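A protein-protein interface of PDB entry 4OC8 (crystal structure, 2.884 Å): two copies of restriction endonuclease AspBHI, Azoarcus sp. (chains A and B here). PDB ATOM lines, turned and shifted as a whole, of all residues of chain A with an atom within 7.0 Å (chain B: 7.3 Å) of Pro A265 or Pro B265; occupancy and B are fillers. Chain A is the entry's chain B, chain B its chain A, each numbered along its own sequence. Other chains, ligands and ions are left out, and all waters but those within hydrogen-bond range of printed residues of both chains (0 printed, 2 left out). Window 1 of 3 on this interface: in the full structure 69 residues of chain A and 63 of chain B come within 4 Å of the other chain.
The side-chain amide nitrogen of Gln B291 is in hydrogen-bond range of the backbone carbonyl oxygen of Leu A262, at 3.4 Å.
The side-chain amide nitrogen of Gln A291 lies within hydrogen-bond range of the backbone carbonyl oxygen of Leu B263 (3.5 Å).
The backbone carbonyl oxygen (O) of Leu B262 lies within hydrogen-bond range of the side-chain amide nitrogen (NE2) of Gln A291 (3.4 Å).
The guanidinium group (NE) of Arg B261 lies within hydrogen-bond range of the backbone carbonyl oxygen (O) of Ala B268 (3.2 Å).
NE of Arg A261 sits at hydrogen-bond distance from O of Ala A268, at 3.1 Å.
OD1 of Asp B266 is in salt-bridge range of NH2 of Arg B288.
Ala A146 touches Arg B261 (CB to O, 3.6 Å).
Gly B290 touches Leu A263.
O of Leu A263 touches NE2 of Gln B291 (3.7 Å).
Ile B289 touches Leu A264.
Leu A264 touches Gly B290 (CD2 to CA, 3.98 Å).
Pro B265 touches Pro A265.
Val A267 touches Ala B146 (CG2 to CB, 3.4 Å).
Leu B264 touches Ile A289 (CD2 to CG2, 3.8 Å).
Gly A290 touches Leu B263.
CD2 of Leu B264 touches CA of Gly A290, 3.9 Å away.
Pro A265 touches just one residue of chain B: Pro B265.
Printed residues of chain B within 4 Å of Leu A287: Ile B289 (3.97 Å).
Of the printed residues of chain B, Gly A290 touches Leu B263 and Leu B264.
Printed residues of chain A within 4 Å of Ala B146: Arg A261 (3.6 Å) and Val A267 (3.4 Å).
Printed residues of chain A within 4 Å of Arg B261: Ala A146 (3.6 Å).
Of the printed residues of chain A, Leu B264 touches Ile A289 and Gly A290.
Of the printed residues of chain A, Pro B265 touches Pro A265 (3.98 Å).
Printed residues of chain A that touch a printed residue of chain B: Ala A146, Arg A261, Leu A262, Leu A263, Leu A264, Pro A265, Val A267, Leu A287, Ile A289, Gly A290 and Gln A291.
Hydrophobic or aromatic side chains of chain A within 4 Å of the printed part of chain B: Ala A146, Leu A263, Leu A264, Pro A265, Val A267, Leu A287 and Ile A289.
Hydrophobic or aromatic side chains of chain B within 4 Å of the printed part of chain A: Ala B146, Leu B263, Leu B264, Pro B265, Val B267 and Ile B289.
Among the printed residues, no Asp or Glu carboxylate lies within 4 Å of a Lys or Arg side-chain nitrogen of the other chain.
Ala A146 touches Arg B261, and with the chains exchanged Arg A261 touches Ala B146.
Leu A264 touches Ile B289, and with the chains exchanged Ile A289 touches Leu B264.
Leu A264 touches Gly B290, and with the chains exchanged Gly A290 touches Leu B264.
Pro B265 touches its own counterpart, Pro A265.
Positions printed for both chains: 146, 260, 261, 262, 263, 264, 265, 266, 267, 268, 287, 288, 289, 290, 291 and 330.
Of the 17 pairs that touch across the chains among the printed residues, 15 have their exchanged pair printed and touching as well.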
ATOM      1  N   ALA A 146     -25.172  25.181 -19.560  1.00  0.00           N
ATOM      2  CA  ALA A 146     -24.476  25.105 -18.279  1.00  0.00           C
ATOM      3  C   ALA A 146     -23.194  25.933 -18.241  1.00  0.00           C
ATOM      4  O   ALA A 146     -22.449  25.889 -17.256  1.00  0.00           O
ATOM      5  CB  ALA A 146     -24.173  23.660 -17.932  1.00  0.00           C
ATOM      6  N   THR A 260      -6.221  14.739  -6.609  1.00  0.00           N
ATOM      7  CA  THR A 260      -7.567  15.059  -6.153  1.00  0.00           C
ATOM      8  C   THR A 260      -7.928  16.489  -6.533  1.00  0.00           C
ATOM      9  O   THR A 260      -9.025  16.745  -7.028  1.00  0.00           O
ATOM     10  CB  THR A 260      -7.723  14.840  -4.631  1.00  0.00           C
ATOM     11  OG1 THR A 260      -7.827  13.436  -4.363  1.00  0.00           O
ATOM     12  CG2 THR A 260      -8.971  15.525  -4.107  1.00  0.00           C
ATOM     13  N   ARG A 261      -6.998  17.417  -6.318  1.00  0.00           N
ATOM     14  CA  ARG A 261      -7.227  18.807  -6.705  1.00  0.00           C
ATOM     15  C   ARG A 261      -7.458  18.920  -8.213  1.00  0.00           C
ATOM     16  O   ARG A 261      -8.134  19.836  -8.670  1.00  0.00           O
ATOM     17  CB  ARG A 261      -6.066  19.701  -6.263  1.00  0.00           C
ATOM     18  CG  ARG A 261      -6.185  20.227  -4.841  1.00  0.00           C
ATOM     19  CD  ARG A 261      -4.921  20.958  -4.423  1.00  0.00           C
ATOM     20  NE  ARG A 261      -5.014  21.530  -3.080  1.00  0.00           N
ATOM     21  CZ  ARG A 261      -4.005  22.128  -2.446  1.00  0.00           C
ATOM     22  NH1 ARG A 261      -2.813  22.234  -3.025  1.00  0.00           N
ATOM     23  NH2 ARG A 261      -4.184  22.621  -1.227  1.00  0.00           N
ATOM     24  N   LEU A 262      -6.883  18.003  -8.985  1.00  0.00           N
ATOM     25  CA  LEU A 262      -7.113  18.001 -10.432  1.00  0.00           C
ATOM     26  C   LEU A 262      -8.479  17.403 -10.784  1.00  0.00           C
ATOM     27  O   LEU A 262      -9.155  17.895 -11.691  1.00  0.00           O
ATOM     28  CB  LEU A 262      -6.004  17.245 -11.162  1.00  0.00           C
ATOM     29  CG  LEU A 262      -4.624  17.903 -11.266  1.00  0.00           C
ATOM     30  CD1 LEU A 262      -3.624  16.975 -11.933  1.00  0.00           C
ATOM     31  CD2 LEU A 262      -4.695  19.219 -12.010  1.00  0.00           C
ATOM     32  N   LEU A 263      -8.869  16.348 -10.065  1.00  0.00           N
ATOM     33  CA  LEU A 263     -10.123  15.627 -10.299  1.00  0.00           C
ATOM     34  C   LEU A 263     -11.336  16.474  -9.910  1.00  0.00           C
ATOM     35  O   LEU A 263     -12.384  16.387 -10.558  1.00  0.00           O
ATOM     36  CB  LEU A 263     -10.135  14.306  -9.507  1.00  0.00           C
ATOM     37  CG  LEU A 263     -11.233  13.267  -9.763  1.00  0.00           C
ATOM     38  CD1 LEU A 263     -10.949  12.480 -11.038  1.00  0.00           C
ATOM     39  CD2 LEU A 263     -11.441  12.308  -8.583  1.00  0.00           C
ATOM     40  N   LEU A 264     -11.178  17.310  -8.879  1.00  0.00           N
ATOM     41  CA  LEU A 264     -12.323  17.956  -8.228  1.00  0.00           C
ATOM     42  C   LEU A 264     -12.566  19.435  -8.579  1.00  0.00           C
ATOM     43  O   LEU A 264     -11.631  20.184  -8.870  1.00  0.00           O
ATOM     44  CB  LEU A 264     -12.282  17.741  -6.697  1.00  0.00           C
ATOM     45  CG  LEU A 264     -12.479  16.289  -6.276  1.00  0.00           C
ATOM     46  CD1 LEU A 264     -12.800  16.093  -4.793  1.00  0.00           C
ATOM     47  CD2 LEU A 264     -13.564  15.722  -7.122  1.00  0.00           C
ATOM     48  N   PRO A 265     -13.845  19.850  -8.549  1.00  0.00           N
ATOM     49  CA  PRO A 265     -14.320  21.124  -9.108  1.00  0.00           C
ATOM     50  C   PRO A 265     -14.033  22.436  -8.340  1.00  0.00           C
ATOM     51  O   PRO A 265     -14.458  23.496  -8.805  1.00  0.00           O
ATOM     52  CB  PRO A 265     -15.834  20.901  -9.250  1.00  0.00           C
ATOM     53  CG  PRO A 265     -16.080  19.448  -8.970  1.00  0.00           C
ATOM     54  CD  PRO A 265     -14.968  19.005  -8.103  1.00  0.00           C
ATOM     55  N   ASP A 266     -13.361  22.384  -7.197  1.00  0.00           N
ATOM     56  CA  ASP A 266     -12.762  23.598  -6.647  1.00  0.00           C
ATOM     57  C   ASP A 266     -11.271  23.304  -6.712  1.00  0.00           C
ATOM     58  O   ASP A 266     -10.827  22.489  -7.528  1.00  0.00           O
ATOM     59  CB  ASP A 266     -13.224  23.839  -5.199  1.00  0.00           C
ATOM     60  CG  ASP A 266     -13.119  25.302  -4.780  1.00  0.00           C
ATOM     61  OD1 ASP A 266     -12.771  26.139  -5.636  1.00  0.00           O
ATOM     62  OD2 ASP A 266     -13.393  25.622  -3.606  1.00  0.00           O
ATOM     63  N   VAL A 267     -10.494  23.975  -5.876  1.00  0.00           N
ATOM     64  CA  VAL A 267      -9.212  23.430  -5.467  1.00  0.00           C
ATOM     65  C   VAL A 267      -9.530  22.948  -4.059  1.00  0.00           C
ATOM     66  O   VAL A 267      -9.747  23.756  -3.162  1.00  0.00           O
ATOM     67  CB  VAL A 267      -8.108  24.492  -5.482  1.00  0.00           C
ATOM     68  CG1 VAL A 267      -6.703  23.854  -5.412  1.00  0.00           C
ATOM     69  CG2 VAL A 267      -8.261  25.364  -6.739  1.00  0.00           C
ATOM     70  N   ALA A 268      -9.641  21.638  -3.875  1.00  0.00           N
ATOM     71  CA  ALA A 268     -10.028  21.117  -2.575  1.00  0.00           C
ATOM     72  C   ALA A 268      -9.025  21.565  -1.519  1.00  0.00           C
ATOM     73  O   ALA A 268      -7.826  21.583  -1.777  1.00  0.00           O
ATOM     74  CB  ALA A 268     -10.127  19.594  -2.622  1.00  0.00           C
ATOM     75  N   LEU A 287     -14.465  20.690  -0.065  1.00  0.00           N
ATOM     76  CA  LEU A 287     -14.818  20.952  -1.449  1.00  0.00           C
ATOM     77  C   LEU A 287     -16.013  21.888  -1.510  1.00  0.00           C
ATOM     78  O   LEU A 287     -16.984  21.715  -0.776  1.00  0.00           O
ATOM     79  CB  LEU A 287     -15.167  19.632  -2.136  1.00  0.00           C
ATOM     80  CG  LEU A 287     -15.604  19.653  -3.598  1.00  0.00           C
ATOM     81  CD1 LEU A 287     -14.444  20.034  -4.502  1.00  0.00           C
ATOM     82  CD2 LEU A 287     -16.162  18.296  -3.975  1.00  0.00           C
ATOM     83  N   ARG A 288     -15.949  22.876  -2.392  1.00  0.00           N
ATOM     84  CA  ARG A 288     -17.039  23.830  -2.516  1.00  0.00           C
ATOM     85  C   ARG A 288     -17.952  23.488  -3.686  1.00  0.00           C
ATOM     86  O   ARG A 288     -17.494  23.307  -4.813  1.00  0.00           O
ATOM     87  CB  ARG A 288     -16.496  25.247  -2.671  1.00  0.00           C
ATOM     88  CG  ARG A 288     -17.395  26.323  -2.093  1.00  0.00           C
ATOM     89  CD  ARG A 288     -16.629  27.622  -1.932  1.00  0.00           C
ATOM     90  NE  ARG A 288     -15.596  27.735  -2.954  1.00  0.00           N
ATOM     91  CZ  ARG A 288     -14.832  28.804  -3.133  1.00  0.00           C
ATOM     92  NH1 ARG A 288     -14.990  29.872  -2.361  1.00  0.00           N
ATOM     93  NH2 ARG A 288     -13.913  28.806  -4.093  1.00  0.00           N
ATOM     94  N   ILE A 289     -19.243  23.385  -3.399  1.00  0.00           N
ATOM     95  CA  ILE A 289     -20.252  23.225  -4.429  1.00  0.00           C
ATOM     96  C   ILE A 289     -20.998  24.541  -4.583  1.00  0.00           C
ATOM     97  O   ILE A 289     -21.574  25.050  -3.617  1.00  0.00           O
ATOM     98  CB  ILE A 289     -21.251  22.119  -4.068  1.00  0.00           C
ATOM     99  CG1 ILE A 289     -20.529  20.775  -3.930  1.00  0.00           C
ATOM    100  CG2 ILE A 289     -22.370  22.048  -5.106  1.00  0.00           C
ATOM    101  CD1 ILE A 289     -21.409  19.659  -3.394  1.00  0.00           C
ATOM    102  N   GLY A 290     -20.975  25.092  -5.794  1.00  0.00           N
ATOM    103  CA  GLY A 290     -21.628  26.355  -6.074  1.00  0.00           C
ATOM    104  C   GLY A 290     -20.630  27.459  -6.361  1.00  0.00           C
ATOM    105  O   GLY A 290     -19.472  27.191  -6.655  1.00  0.00           O
ATOM    106  N   GLN A 291     -21.088  28.703  -6.293  1.00  0.00           N
ATOM    107  CA  GLN A 291     -20.219  29.859  -6.480  1.00  0.00           C
ATOM    108  C   GLN A 291     -20.535  30.899  -5.409  1.00  0.00           C
ATOM    109  O   GLN A 291     -21.631  31.456  -5.399  1.00  0.00           O
ATOM    110  CB  GLN A 291     -20.419  30.467  -7.874  1.00  0.00           C
ATOM    111  CG  GLN A 291     -20.261  29.480  -9.026  1.00  0.00           C
ATOM    112  CD  GLN A 291     -20.562  30.101 -10.385  1.00  0.00           C
ATOM    113  OE1 GLN A 291     -20.403  31.308 -10.583  1.00  0.00           O
ATOM    114  NE2 GLN A 291     -21.004  29.274 -11.329  1.00  0.00           N
ATOM    115  N   PHE A 330     -18.558  12.452   1.366  1.00  0.00           N
ATOM    116  CA  PHE A 330     -18.073  11.390   0.493  1.00  0.00           C
ATOM    117  C   PHE A 330     -16.611  11.021   0.719  1.00  0.00           C
ATOM    118  O   PHE A 330     -15.965  11.507   1.646  1.00  0.00           O
ATOM    119  CB  PHE A 330     -18.325  11.733  -0.982  1.00  0.00           C
ATOM    120  CG  PHE A 330     -17.492  12.871  -1.502  1.00  0.00           C
ATOM    121  CD1 PHE A 330     -17.820  14.184  -1.208  1.00  0.00           C
ATOM    122  CD2 PHE A 330     -16.399  12.629  -2.313  1.00  0.00           C
ATOM    123  CE1 PHE A 330     -17.061  15.237  -1.699  1.00  0.00           C
ATOM    124  CE2 PHE A 330     -15.636  13.677  -2.809  1.00  0.00           C
ATOM    125  CZ  PHE A 330     -15.968  14.982  -2.501  1.00  0.00           C
ATOM    126  N   ALA B 146      -4.937  23.341  -9.964  1.00  0.00           N
ATOM    127  CA  ALA B 146      -6.230  22.689 -10.187  1.00  0.00           C
ATOM    128  C   ALA B 146      -6.708  22.728 -11.639  1.00  0.00           C
ATOM    129  O   ALA B 146      -7.738  22.139 -11.976  1.00  0.00           O
ATOM    130  CB  ALA B 146      -7.285  23.278  -9.281  1.00  0.00           C
ATOM    131  N   THR B 260     -29.884  26.911 -11.798  1.00  0.00           N
ATOM    132  CA  THR B 260     -29.119  25.912 -11.073  1.00  0.00           C
ATOM    133  C   THR B 260     -28.043  25.332 -11.985  1.00  0.00           C
ATOM    134  O   THR B 260     -26.885  25.233 -11.586  1.00  0.00           O
ATOM    135  CB  THR B 260     -30.028  24.816 -10.481  1.00  0.00           C
ATOM    136  OG1 THR B 260     -30.709  25.340  -9.333  1.00  0.00           O
ATOM    137  CG2 THR B 260     -29.225  23.600 -10.060  1.00  0.00           C
ATOM    138  N   ARG B 261     -28.408  25.021 -13.228  1.00  0.00           N
ATOM    139  CA  ARG B 261     -27.447  24.424 -14.145  1.00  0.00           C
ATOM    140  C   ARG B 261     -26.261  25.359 -14.361  1.00  0.00           C
ATOM    141  O   ARG B 261     -25.157  24.899 -14.647  1.00  0.00           O
ATOM    142  CB  ARG B 261     -28.109  24.057 -15.477  1.00  0.00           C
ATOM    143  CG  ARG B 261     -28.893  22.759 -15.433  1.00  0.00           C
ATOM    144  CD  ARG B 261     -29.535  22.472 -16.769  1.00  0.00           C
ATOM    145  NE  ARG B 261     -30.330  21.245 -16.768  1.00  0.00           N
ATOM    146  CZ  ARG B 261     -31.112  20.869 -17.778  1.00  0.00           C
ATOM    147  NH1 ARG B 261     -31.205  21.631 -18.861  1.00  0.00           N
ATOM    148  NH2 ARG B 261     -31.806  19.739 -17.708  1.00  0.00           N
ATOM    149  N   LEU B 262     -26.488  26.665 -14.224  1.00  0.00           N
ATOM    150  CA  LEU B 262     -25.426  27.640 -14.439  1.00  0.00           C
ATOM    151  C   LEU B 262     -24.562  27.686 -13.191  1.00  0.00           C
ATOM    152  O   LEU B 262     -23.340  27.799 -13.272  1.00  0.00           O
ATOM    153  CB  LEU B 262     -26.020  29.018 -14.706  1.00  0.00           C
ATOM    154  CG  LEU B 262     -26.596  29.277 -16.095  1.00  0.00           C
ATOM    155  CD1 LEU B 262     -27.261  30.651 -16.181  1.00  0.00           C
ATOM    156  CD2 LEU B 262     -25.514  29.141 -17.149  1.00  0.00           C
ATOM    157  N   LEU B 263     -25.214  27.572 -12.036  1.00  0.00           N
ATOM    158  CA  LEU B 263     -24.540  27.681 -10.750  1.00  0.00           C
ATOM    159  C   LEU B 263     -23.661  26.472 -10.427  1.00  0.00           C
ATOM    160  O   LEU B 263     -22.625  26.627  -9.758  1.00  0.00           O
ATOM    161  CB  LEU B 263     -25.568  27.887  -9.625  1.00  0.00           C
ATOM    162  CG  LEU B 263     -25.010  28.051  -8.210  1.00  0.00           C
ATOM    163  CD1 LEU B 263     -24.541  29.479  -7.982  1.00  0.00           C
ATOM    164  CD2 LEU B 263     -25.989  27.617  -7.113  1.00  0.00           C
ATOM    165  N   LEU B 264     -24.055  25.299 -10.938  1.00  0.00           N
ATOM    166  CA  LEU B 264     -23.536  24.008 -10.467  1.00  0.00           C
ATOM    167  C   LEU B 264     -22.642  23.260 -11.455  1.00  0.00           C
ATOM    168  O   LEU B 264     -22.865  23.327 -12.663  1.00  0.00           O
ATOM    169  CB  LEU B 264     -24.720  23.101  -9.996  1.00  0.00           C
ATOM    170  CG  LEU B 264     -25.374  23.637  -8.740  1.00  0.00           C
ATOM    171  CD1 LEU B 264     -26.354  22.717  -8.017  1.00  0.00           C
ATOM    172  CD2 LEU B 264     -24.262  23.998  -7.818  1.00  0.00           C
ATOM    173  N   PRO B 265     -21.641  22.540 -10.928  1.00  0.00           N
ATOM    174  CA  PRO B 265     -20.464  22.028 -11.629  1.00  0.00           C
ATOM    175  C   PRO B 265     -20.691  20.864 -12.608  1.00  0.00           C
ATOM    176  O   PRO B 265     -19.730  20.235 -13.056  1.00  0.00           O
ATOM    177  CB  PRO B 265     -19.550  21.579 -10.493  1.00  0.00           C
ATOM    178  CG  PRO B 265     -20.186  21.982  -9.220  1.00  0.00           C
ATOM    179  CD  PRO B 265     -21.612  22.214  -9.498  1.00  0.00           C
ATOM    180  N   ASP B 266     -21.939  20.604 -12.957  1.00  0.00           N
ATOM    181  CA  ASP B 266     -22.266  19.585 -13.936  1.00  0.00           C
ATOM    182  C   ASP B 266     -23.084  20.317 -14.973  1.00  0.00           C
ATOM    183  O   ASP B 266     -22.838  21.481 -15.273  1.00  0.00           O
ATOM    184  CB  ASP B 266     -23.159  18.530 -13.263  1.00  0.00           C
ATOM    185  CG  ASP B 266     -22.893  17.100 -13.744  1.00  0.00           C
ATOM    186  OD1 ASP B 266     -22.358  16.919 -14.860  1.00  0.00           O
ATOM    187  OD2 ASP B 266     -23.254  16.165 -13.005  1.00  0.00           O
ATOM    188  N   VAL B 267     -24.041  19.604 -15.540  1.00  0.00           N
ATOM    189  CA  VAL B 267     -25.275  20.204 -15.969  1.00  0.00           C
ATOM    190  C   VAL B 267     -26.173  19.324 -15.083  1.00  0.00           C
ATOM    191  O   VAL B 267     -26.212  18.107 -15.271  1.00  0.00           O
ATOM    192  CB  VAL B 267     -25.523  19.973 -17.474  1.00  0.00           C
ATOM    193  CG1 VAL B 267     -26.549  20.929 -18.038  1.00  0.00           C
ATOM    194  CG2 VAL B 267     -24.213  20.130 -18.223  1.00  0.00           C
ATOM    195  N   ALA B 268     -26.841  19.895 -14.082  1.00  0.00           N
ATOM    196  CA  ALA B 268     -27.580  19.058 -13.151  1.00  0.00           C
ATOM    197  C   ALA B 268     -28.693  18.348 -13.917  1.00  0.00           C
ATOM    198  O   ALA B 268     -29.333  18.936 -14.798  1.00  0.00           O
ATOM    199  CB  ALA B 268     -28.147  19.888 -11.995  1.00  0.00           C
ATOM    200  N   LEU B 287     -26.345  15.458  -9.445  1.00  0.00           N
ATOM    201  CA  LEU B 287     -25.082  16.143  -9.696  1.00  0.00           C
ATOM    202  C   LEU B 287     -23.921  15.156  -9.683  1.00  0.00           C
ATOM    203  O   LEU B 287     -23.865  14.266  -8.844  1.00  0.00           O
ATOM    204  CB  LEU B 287     -24.853  17.208  -8.623  1.00  0.00           C
ATOM    205  CG  LEU B 287     -23.530  17.968  -8.634  1.00  0.00           C
ATOM    206  CD1 LEU B 287     -23.471  18.891  -9.827  1.00  0.00           C
ATOM    207  CD2 LEU B 287     -23.354  18.746  -7.339  1.00  0.00           C
ATOM    208  N   ARG B 288     -22.989  15.317 -10.611  1.00  0.00           N
ATOM    209  CA  ARG B 288     -21.821  14.446 -10.659  1.00  0.00           C
ATOM    210  C   ARG B 288     -20.628  15.170 -10.056  1.00  0.00           C
ATOM    211  O   ARG B 288     -20.396  16.340 -10.335  1.00  0.00           O
ATOM    212  CB  ARG B 288     -21.523  14.042 -12.101  1.00  0.00           C
ATOM    213  CG  ARG B 288     -20.643  12.849 -12.284  1.00  0.00           C
ATOM    214  CD  ARG B 288     -20.797  12.310 -13.702  1.00  0.00           C
ATOM    215  NE  ARG B 288     -20.935  13.400 -14.663  1.00  0.00           N
ATOM    216  CZ  ARG B 288     -21.073  13.237 -15.975  1.00  0.00           C
ATOM    217  NH1 ARG B 288     -21.088  12.021 -16.504  1.00  0.00           N
ATOM    218  NH2 ARG B 288     -21.189  14.299 -16.758  1.00  0.00           N
ATOM    219  N   ILE B 289     -19.896  14.477  -9.195  1.00  0.00           N
ATOM    220  CA  ILE B 289     -18.694  15.021  -8.595  1.00  0.00           C
ATOM    221  C   ILE B 289     -17.534  14.156  -9.045  1.00  0.00           C
ATOM    222  O   ILE B 289     -17.536  12.936  -8.825  1.00  0.00           O
ATOM    223  CB  ILE B 289     -18.774  15.008  -7.066  1.00  0.00           C
ATOM    224  CG1 ILE B 289     -19.918  15.896  -6.591  1.00  0.00           C
ATOM    225  CG2 ILE B 289     -17.465  15.476  -6.452  1.00  0.00           C
ATOM    226  CD1 ILE B 289     -20.096  15.886  -5.087  1.00  0.00           C
ATOM    227  N   GLY B 290     -16.555  14.786  -9.687  1.00  0.00           N
ATOM    228  CA  GLY B 290     -15.418  14.075 -10.235  1.00  0.00           C
ATOM    229  C   GLY B 290     -15.409  14.093 -11.748  1.00  0.00           C
ATOM    230  O   GLY B 290     -16.040  14.938 -12.373  1.00  0.00           O
ATOM    231  N   GLN B 291     -14.666  13.167 -12.339  1.00  0.00           N
ATOM    232  CA  GLN B 291     -14.602  13.045 -13.785  1.00  0.00           C
ATOM    233  C   GLN B 291     -14.692  11.577 -14.168  1.00  0.00           C
ATOM    234  O   GLN B 291     -13.758  10.817 -13.927  1.00  0.00           O
ATOM    235  CB  GLN B 291     -13.301  13.642 -14.327  1.00  0.00           C
ATOM    236  CG  GLN B 291     -13.121  15.124 -14.052  1.00  0.00           C
ATOM    237  CD  GLN B 291     -11.874  15.686 -14.715  1.00  0.00           C
ATOM    238  OE1 GLN B 291     -11.490  15.253 -15.804  1.00  0.00           O
ATOM    239  NE2 GLN B 291     -11.227  16.649 -14.055  1.00  0.00           N
ATOM    240  N   PHE B 330     -27.796  17.476  -0.393  1.00  0.00           N
ATOM    241  CA  PHE B 330     -27.973  18.903  -0.142  1.00  0.00           C
ATOM    242  C   PHE B 330     -29.227  19.508  -0.786  1.00  0.00           C
ATOM    243  O   PHE B 330     -30.017  18.811  -1.426  1.00  0.00           O
ATOM    244  CB  PHE B 330     -26.720  19.677  -0.560  1.00  0.00           C
ATOM    245  CG  PHE B 330     -26.452  19.660  -2.038  1.00  0.00           C
ATOM    246  CD1 PHE B 330     -25.890  18.543  -2.645  1.00  0.00           C
ATOM    247  CD2 PHE B 330     -26.744  20.768  -2.818  1.00  0.00           C
ATOM    248  CE1 PHE B 330     -25.635  18.529  -4.005  1.00  0.00           C
ATOM    249  CE2 PHE B 330     -26.491  20.763  -4.174  1.00  0.00           C
ATOM    250  CZ  PHE B 330     -25.933  19.642  -4.771  1.00  0.00           C
